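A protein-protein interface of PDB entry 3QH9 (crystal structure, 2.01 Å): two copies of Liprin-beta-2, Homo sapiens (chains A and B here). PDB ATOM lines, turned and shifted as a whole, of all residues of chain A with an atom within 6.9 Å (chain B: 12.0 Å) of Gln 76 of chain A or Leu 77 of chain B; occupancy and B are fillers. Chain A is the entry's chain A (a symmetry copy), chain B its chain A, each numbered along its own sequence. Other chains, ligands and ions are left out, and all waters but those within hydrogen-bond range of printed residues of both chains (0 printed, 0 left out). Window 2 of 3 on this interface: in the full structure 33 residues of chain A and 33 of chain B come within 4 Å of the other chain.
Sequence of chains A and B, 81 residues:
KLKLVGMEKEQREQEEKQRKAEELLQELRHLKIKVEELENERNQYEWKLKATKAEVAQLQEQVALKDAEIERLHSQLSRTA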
ATOM      1  N   GLU A  71      -0.051 -22.503  -2.233  1.00  0.00           N
ATOM      2  CA  GLU A  71      -1.273 -22.736  -2.987  1.00  0.00           C
ATOM      3  C   GLU A  71      -1.979 -21.426  -3.370  1.00  0.00           C
ATOM      4  O   GLU A  71      -2.474 -21.242  -4.477  1.00  0.00           O
ATOM      5  CB  GLU A  71      -2.258 -23.624  -2.179  1.00  0.00           C
ATOM      6  CG  GLU A  71      -1.953 -25.167  -2.153  1.00  0.00           C
ATOM      7  CD  GLU A  71      -2.162 -25.886  -0.766  1.00  0.00           C
ATOM      8  OE1 GLU A  71      -2.961 -25.397   0.064  1.00  0.00           O
ATOM      9  OE2 GLU A  71      -1.516 -26.947  -0.477  1.00  0.00           O
ATOM     10  N   ARG A  72      -2.022 -20.473  -2.464  1.00  0.00           N
ATOM     11  CA  ARG A  72      -2.648 -19.238  -2.787  1.00  0.00           C
ATOM     12  C   ARG A  72      -1.944 -18.551  -3.926  1.00  0.00           C
ATOM     13  O   ARG A  72      -2.637 -18.063  -4.866  1.00  0.00           O
ATOM     14  CB  ARG A  72      -2.759 -18.339  -1.553  1.00  0.00           C
ATOM     15  CG  ARG A  72      -3.425 -17.015  -1.772  1.00  0.00           C
ATOM     16  CD  ARG A  72      -3.456 -16.192  -0.496  1.00  0.00           C
ATOM     17  NE  ARG A  72      -2.174 -15.540  -0.302  1.00  0.00           N
ATOM     18  CZ  ARG A  72      -1.794 -14.449  -0.965  1.00  0.00           C
ATOM     19  NH1 ARG A  72      -2.627 -13.884  -1.830  1.00  0.00           N
ATOM     20  NH2 ARG A  72      -0.579 -13.907  -0.753  1.00  0.00           N
ATOM     21  N   LEU A  73      -0.609 -18.483  -3.846  1.00  0.00           N
ATOM     22  CA  LEU A  73       0.246 -17.895  -4.895  1.00  0.00           C
ATOM     23  C   LEU A  73       0.124 -18.619  -6.226  1.00  0.00           C
ATOM     24  O   LEU A  73       0.022 -17.966  -7.254  1.00  0.00           O
ATOM     25  CB  LEU A  73       1.735 -17.840  -4.481  1.00  0.00           C
ATOM     26  CG  LEU A  73       2.076 -17.078  -3.203  1.00  0.00           C
ATOM     27  CD1 LEU A  73       3.579 -17.179  -2.831  1.00  0.00           C
ATOM     28  CD2 LEU A  73       1.600 -15.659  -3.319  1.00  0.00           C
ATOM     29  N   HIS A  74       0.166 -19.940  -6.228  1.00  0.00           N
ATOM     30  CA  HIS A  74      -0.081 -20.683  -7.437  1.00  0.00           C
ATOM     31  C   HIS A  74      -1.439 -20.423  -8.120  1.00  0.00           C
ATOM     32  O   HIS A  74      -1.503 -20.400  -9.364  1.00  0.00           O
ATOM     33  CB  HIS A  74       0.138 -22.187  -7.208  1.00  0.00           C
ATOM     34  CG  HIS A  74       1.592 -22.592  -7.143  1.00  0.00           C
ATOM     35  ND1 HIS A  74       2.034 -23.704  -6.455  1.00  0.00           N
ATOM     36  CD2 HIS A  74       2.701 -22.037  -7.696  1.00  0.00           C
ATOM     37  CE1 HIS A  74       3.348 -23.812  -6.574  1.00  0.00           C
ATOM     38  NE2 HIS A  74       3.778 -22.812  -7.326  1.00  0.00           N
ATOM     39  N   SER A  75      -2.527 -20.251  -7.364  1.00  0.00           N
ATOM     40  CA  SER A  75      -3.820 -19.803  -7.995  1.00  0.00           C
ATOM     41  C   SER A  75      -3.716 -18.466  -8.721  1.00  0.00           C
ATOM     42  O   SER A  75      -4.227 -18.269  -9.860  1.00  0.00           O
ATOM     43  CB  SER A  75      -4.922 -19.671  -6.940  1.00  0.00           C
ATOM     44  OG  SER A  75      -5.202 -20.948  -6.411  1.00  0.00           O
ATOM     45  N   GLN A  76      -3.070 -17.520  -8.042  1.00  0.00           N
ATOM     46  CA  GLN A  76      -2.861 -16.230  -8.630  1.00  0.00           C
ATOM     47  C   GLN A  76      -1.966 -16.336  -9.860  1.00  0.00           C
ATOM     48  O   GLN A  76      -2.317 -15.910 -10.960  1.00  0.00           O
ATOM     49  CB  GLN A  76      -2.177 -15.306  -7.661  1.00  0.00           C
ATOM     50  CG  GLN A  76      -2.980 -14.854  -6.487  1.00  0.00           C
ATOM     51  CD  GLN A  76      -2.222 -13.751  -5.734  1.00  0.00           C
ATOM     52  OE1 GLN A  76      -1.193 -13.262  -6.187  1.00  0.00           O
ATOM     53  NE2 GLN A  76      -2.741 -13.353  -4.620  1.00  0.00           N
ATOM     54  N   LEU A  77      -0.789 -16.900  -9.673  1.00  0.00           N
ATOM     55  CA  LEU A  77       0.203 -17.074 -10.745  1.00  0.00           C
ATOM     56  C   LEU A  77      -0.437 -17.649 -12.001  1.00  0.00           C
ATOM     57  O   LEU A  77      -0.067 -17.309 -13.133  1.00  0.00           O
ATOM     58  CB  LEU A  77       1.375 -17.980 -10.274  1.00  0.00           C
ATOM     59  CG  LEU A  77       1.933 -19.127 -11.144  1.00  0.00           C
ATOM     60  CD1 LEU A  77       3.308 -19.515 -10.660  1.00  0.00           C
ATOM     61  CD2 LEU A  77       1.011 -20.353 -11.137  1.00  0.00           C
ATOM     62  N   SER A  78      -1.399 -18.568 -11.817  1.00  0.00           N
ATOM     63  CA  SER A  78      -2.001 -19.238 -12.981  1.00  0.00           C
ATOM     64  C   SER A  78      -3.189 -18.492 -13.663  1.00  0.00           C
ATOM     65  O   SER A  78      -3.688 -18.975 -14.696  1.00  0.00           O
ATOM     66  CB  SER A  78      -2.365 -20.691 -12.657  1.00  0.00           C
ATOM     67  OG  SER A  78      -3.390 -20.782 -11.690  1.00  0.00           O
ATOM     68  N   ARG A  79      -3.608 -17.324 -13.146  1.00  0.00           N
ATOM     69  CA  ARG A  79      -4.694 -16.536 -13.768  1.00  0.00           C
ATOM     70  C   ARG A  79      -4.243 -15.885 -15.097  1.00  0.00           C
ATOM     71  O   ARG A  79      -3.059 -15.551 -15.295  1.00  0.00           O
ATOM     72  CB  ARG A  79      -5.244 -15.466 -12.786  1.00  0.00           C
ATOM     73  CG  ARG A  79      -6.199 -16.005 -11.682  1.00  0.00           C
ATOM     74  CD  ARG A  79      -6.338 -15.049 -10.464  1.00  0.00           C
ATOM     75  NE  ARG A  79      -6.769 -15.761  -9.256  1.00  0.00           N
ATOM     76  CZ  ARG A  79      -6.736 -15.275  -8.006  1.00  0.00           C
ATOM     77  NH1 ARG A  79      -6.325 -14.036  -7.748  1.00  0.00           N
ATOM     78  NH2 ARG A  79      -7.156 -16.026  -6.986  1.00  0.00           N
ATOM     79  N   ALA B  68      11.778 -20.628   0.614  1.00  0.00           N
ATOM     80  CA  ALA B  68      12.450 -20.368  -0.688  1.00  0.00           C
ATOM     81  C   ALA B  68      11.470 -20.347  -1.906  1.00  0.00           C
ATOM     82  O   ALA B  68      11.615 -19.592  -2.936  1.00  0.00           O
ATOM     83  CB  ALA B  68      13.595 -21.413  -0.881  1.00  0.00           C
ATOM     84  N   GLU B  69      10.503 -21.235  -1.810  1.00  0.00           N
ATOM     85  CA  GLU B  69       9.502 -21.350  -2.849  1.00  0.00           C
ATOM     86  C   GLU B  69       8.529 -20.173  -2.796  1.00  0.00           C
ATOM     87  O   GLU B  69       8.206 -19.624  -3.853  1.00  0.00           O
ATOM     88  CB  GLU B  69       8.815 -22.738  -2.862  1.00  0.00           C
ATOM     89  CG  GLU B  69       7.682 -22.889  -3.951  1.00  0.00           C
ATOM     90  CD  GLU B  69       8.217 -22.997  -5.410  1.00  0.00           C
ATOM     91  OE1 GLU B  69       7.422 -23.191  -6.408  1.00  0.00           O
ATOM     92  OE2 GLU B  69       9.460 -22.924  -5.530  1.00  0.00           O
ATOM     93  N   ILE B  70       8.146 -19.724  -1.605  1.00  0.00           N
ATOM     94  CA  ILE B  70       7.331 -18.510  -1.469  1.00  0.00           C
ATOM     95  C   ILE B  70       8.091 -17.262  -2.005  1.00  0.00           C
ATOM     96  O   ILE B  70       7.525 -16.431  -2.740  1.00  0.00           O
ATOM     97  CB  ILE B  70       6.861 -18.291  -0.028  1.00  0.00           C
ATOM     98  CG1 ILE B  70       5.841 -19.339   0.429  1.00  0.00           C
ATOM     99  CG2 ILE B  70       6.301 -16.914   0.145  1.00  0.00           C
ATOM    100  CD1 ILE B  70       5.736 -19.480   1.905  1.00  0.00           C
ATOM    101  N   GLU B  71       9.364 -17.125  -1.684  1.00  0.00           N
ATOM    102  CA  GLU B  71      10.173 -16.040  -2.215  1.00  0.00           C
ATOM    103  C   GLU B  71      10.264 -16.079  -3.748  1.00  0.00           C
ATOM    104  O   GLU B  71      10.185 -15.070  -4.440  1.00  0.00           O
ATOM    105  CB  GLU B  71      11.609 -16.082  -1.621  1.00  0.00           C
ATOM    106  CG  GLU B  71      11.779 -15.525  -0.159  1.00  0.00           C
ATOM    107  CD  GLU B  71      12.735 -16.352   0.783  1.00  0.00           C
ATOM    108  OE1 GLU B  71      13.638 -17.056   0.277  1.00  0.00           O
ATOM    109  OE2 GLU B  71      12.587 -16.323   2.050  1.00  0.00           O
ATOM    110  N   ARG B  72      10.416 -17.255  -4.317  1.00  0.00           N
ATOM    111  CA  ARG B  72      10.484 -17.336  -5.735  1.00  0.00           C
ATOM    112  C   ARG B  72       9.211 -16.845  -6.370  1.00  0.00           C
ATOM    113  O   ARG B  72       9.287 -16.056  -7.356  1.00  0.00           O
ATOM    114  CB  ARG B  72      10.846 -18.752  -6.188  1.00  0.00           C
ATOM    115  CG  ARG B  72      10.967 -18.949  -7.668  1.00  0.00           C
ATOM    116  CD  ARG B  72      11.297 -20.392  -8.010  1.00  0.00           C
ATOM    117  NE  ARG B  72      10.087 -21.191  -7.981  1.00  0.00           N
ATOM    118  CZ  ARG B  72       9.181 -21.195  -8.958  1.00  0.00           C
ATOM    119  NH1 ARG B  72       9.388 -20.464 -10.046  1.00  0.00           N
ATOM    120  NH2 ARG B  72       8.067 -21.945  -8.856  1.00  0.00           N
ATOM    121  N   LEU B  73       8.070 -17.311  -5.850  1.00  0.00           N
ATOM    122  CA  LEU B  73       6.729 -16.898  -6.311  1.00  0.00           C
ATOM    123  C   LEU B  73       6.481 -15.408  -6.134  1.00  0.00           C
ATOM    124  O   LEU B  73       5.963 -14.777  -7.042  1.00  0.00           O
ATOM    125  CB  LEU B  73       5.596 -17.688  -5.617  1.00  0.00           C
ATOM    126  CG  LEU B  73       5.622 -19.208  -5.753  1.00  0.00           C
ATOM    127  CD1 LEU B  73       4.501 -19.898  -4.931  1.00  0.00           C
ATOM    128  CD2 LEU B  73       5.595 -19.587  -7.205  1.00  0.00           C
ATOM    129  N   HIS B  74       6.809 -14.850  -4.981  1.00  0.00           N
ATOM    130  CA  HIS B  74       6.726 -13.424  -4.803  1.00  0.00           C
ATOM    131  C   HIS B  74       7.548 -12.574  -5.793  1.00  0.00           C
ATOM    132  O   HIS B  74       7.079 -11.496  -6.209  1.00  0.00           O
ATOM    133  CB  HIS B  74       7.046 -13.035  -3.351  1.00  0.00           C
ATOM    134  CG  HIS B  74       5.924 -13.318  -2.379  1.00  0.00           C
ATOM    135  ND1 HIS B  74       6.132 -13.554  -1.035  1.00  0.00           N
ATOM    136  CD2 HIS B  74       4.579 -13.386  -2.560  1.00  0.00           C
ATOM    137  CE1 HIS B  74       4.974 -13.767  -0.432  1.00  0.00           C
ATOM    138  NE2 HIS B  74       4.013 -13.668  -1.336  1.00  0.00           N
ATOM    139  N   SER B  75       8.757 -12.998  -6.170  1.00  0.00           N
ATOM    140  CA  SER B  75       9.492 -12.292  -7.279  1.00  0.00           C
ATOM    141  C   SER B  75       8.731 -12.270  -8.601  1.00  0.00           C
ATOM    142  O   SER B  75       8.647 -11.234  -9.320  1.00  0.00           O
ATOM    143  CB  SER B  75      10.848 -12.952  -7.538  1.00  0.00           C
ATOM    144  OG  SER B  75      11.664 -12.781  -6.399  1.00  0.00           O
ATOM    145  N   GLN B  76       8.192 -13.438  -8.944  1.00  0.00           N
ATOM    146  CA  GLN B  76       7.412 -13.544 -10.141  1.00  0.00           C
ATOM    147  C   GLN B  76       6.155 -12.688 -10.043  1.00  0.00           C
ATOM    148  O   GLN B  76       5.884 -11.828 -10.881  1.00  0.00           O
ATOM    149  CB  GLN B  76       6.968 -14.963 -10.365  1.00  0.00           C
ATOM    150  CG  GLN B  76       8.026 -15.946 -10.738  1.00  0.00           C
ATOM    151  CD  GLN B  76       7.377 -17.276 -11.149  1.00  0.00           C
ATOM    152  OE1 GLN B  76       6.163 -17.380 -11.276  1.00  0.00           O
ATOM    153  NE2 GLN B  76       8.181 -18.262 -11.377  1.00  0.00           N
ATOM    154  N   LEU B  77       5.367 -12.931  -9.014  1.00  0.00           N
ATOM    155  CA  LEU B  77       4.109 -12.208  -8.768  1.00  0.00           C
ATOM    156  C   LEU B  77       4.301 -10.704  -8.913  1.00  0.00           C
ATOM    157  O   LEU B  77       3.416  -9.979  -9.387  1.00  0.00           O
ATOM    158  CB  LEU B  77       3.539 -12.546  -7.363  1.00  0.00           C
ATOM    159  CG  LEU B  77       3.010 -11.459  -6.403  1.00  0.00           C
ATOM    160  CD1 LEU B  77       2.126 -12.088  -5.354  1.00  0.00           C
ATOM    161  CD2 LEU B  77       4.150 -10.685  -5.729  1.00  0.00           C
ATOM    162  N   SER B  78       5.465 -10.203  -8.468  1.00  0.00           N
ATOM    163  CA  SER B  78       5.687  -8.748  -8.487  1.00  0.00           C
ATOM    164  C   SER B  78       6.228  -8.155  -9.824  1.00  0.00           C
ATOM    165  O   SER B  78       6.365  -6.921  -9.922  1.00  0.00           O
ATOM    166  CB  SER B  78       6.538  -8.302  -7.292  1.00  0.00           C
ATOM    167  OG  SER B  78       7.853  -8.812  -7.353  1.00  0.00           O
ATOM    168  N   ARG B  79       6.485  -8.985 -10.850  1.00  0.00           N
ATOM    169  CA  ARG B  79       6.949  -8.489 -12.163  1.00  0.00           C
ATOM    170  C   ARG B  79       5.827  -7.751 -12.929  1.00  0.00           C
ATOM    171  O   ARG B  79       4.627  -8.050 -12.783  1.00  0.00           O
ATOM    172  CB  ARG B  79       7.541  -9.642 -13.020  1.00  0.00           C
ATOM    173  CG  ARG B  79       8.975 -10.096 -12.626  1.00  0.00           C
ATOM    174  CD  ARG B  79       9.339 -11.516 -13.145  1.00  0.00           C
ATOM    175  NE  ARG B  79      10.411 -12.131 -12.354  1.00  0.00           N
ATOM    176  CZ  ARG B  79      10.766 -13.423 -12.388  1.00  0.00           C
ATOM    177  NH1 ARG B  79      10.176 -14.291 -13.206  1.00  0.00           N
ATOM    178  NH2 ARG B  79      11.761 -13.862 -11.614  1.00  0.00           N
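The guanidinium group of Arg 72 of chain B lies within salt-bridge range of the side-chain carboxylate of Glu 69 of chain B, at 2.8 Å.
The guanidinium group of Arg 72 of chain B sits close to the side-chain amide nitrogen of Gln 76 of chain B, at 2.8 Å.
The side-chain hydroxyl (OG) of Ser 78 of chain B is in hydrogen-bond range of the backbone carbonyl oxygen (O) of His 74 of chain B (3.0 Å).
The side-chain amide nitrogen (NE2) of Gln 76 of chain A sits close to the guanidinium group (NH1) of Arg 72 of chain A.
OG of Ser 78 of chain A sits at hydrogen-bond distance from O of His 74 of chain A (3.0 Å).
Among the printed residues, pairs that only touch across the chains: Leu 73 of chain A with Leu 73 of chain B (3.5 Å), Gln 76 of chain A with Leu 77 of chain B (3.6 Å), Leu 77 of chain A with Gln 76 of chain B (3.6 Å), His 74 of chain A with Leu 73 of chain B (3.7 Å), Leu 73 of chain A with His 74 of chain B (3.7 Å) and His 74 of chain A with Glu 69 of chain B (3.8 Å).
Printed residues of chain B within 4 Å of Gln 76 of chain A: Leu 77.
Of the printed residues of chain A, Leu 77 of chain B touches Gln 76 (3.6 Å).
No residue of chain B comes within 4 Å of Ser 75 of chain A.
No residue of chain B comes within 4 Å of Ser 78 of chain A.
Of the printed residues of chain B, Leu 73 of chain A touches Leu 73 and His 74.
Printed residues of chain B within 4 Å of Leu 77 of chain A: Gln 76 (3.6 Å).
Of the printed residues of chain B, His 74 of chain A touches Glu 69 and Leu 73.
Printed residues of chain A within 4 Å of Glu 69 of chain B: His 74 (3.8 Å).
Glu 71 of chain A touches none of the printed residues of chain B.
The nearest printed residue of chain B that does not touch Gln 76 of chain A is His 74 of chain B (6.8 Å).
The nearest printed residue of chain A that does not touch Leu 77 of chain B is Leu 73 of chain A (4.1 Å).
Printed residues of chain A that touch a printed residue of chain B: Leu 73, His 74, Gln 76 and Leu 77.
Hydrophobic or aromatic side chains of chain A that line the printed part of chain B: Leu 73, His 74 and Leu 77.
Hydrophobic or aromatic side chains of chain B within 4 Å of the printed part of chain A: Leu 73, His 74 and Leu 77.
Among the printed residues, no Asp or Glu carboxylate lies within 4 Å of a Lys or Arg side-chain nitrogen of the other chain.
Leu 73 of chain B touches its own counterpart, Leu 73 of chain A.
Leu 73 of chain A touches His 74 of chain B, and with the chains exchanged His 74 of chain A touches Leu 73 of chain B.
Gln 76 of chain A touches Leu 77 of chain B, and with the chains exchanged Leu 77 of chain A touches Gln 76 of chain B.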
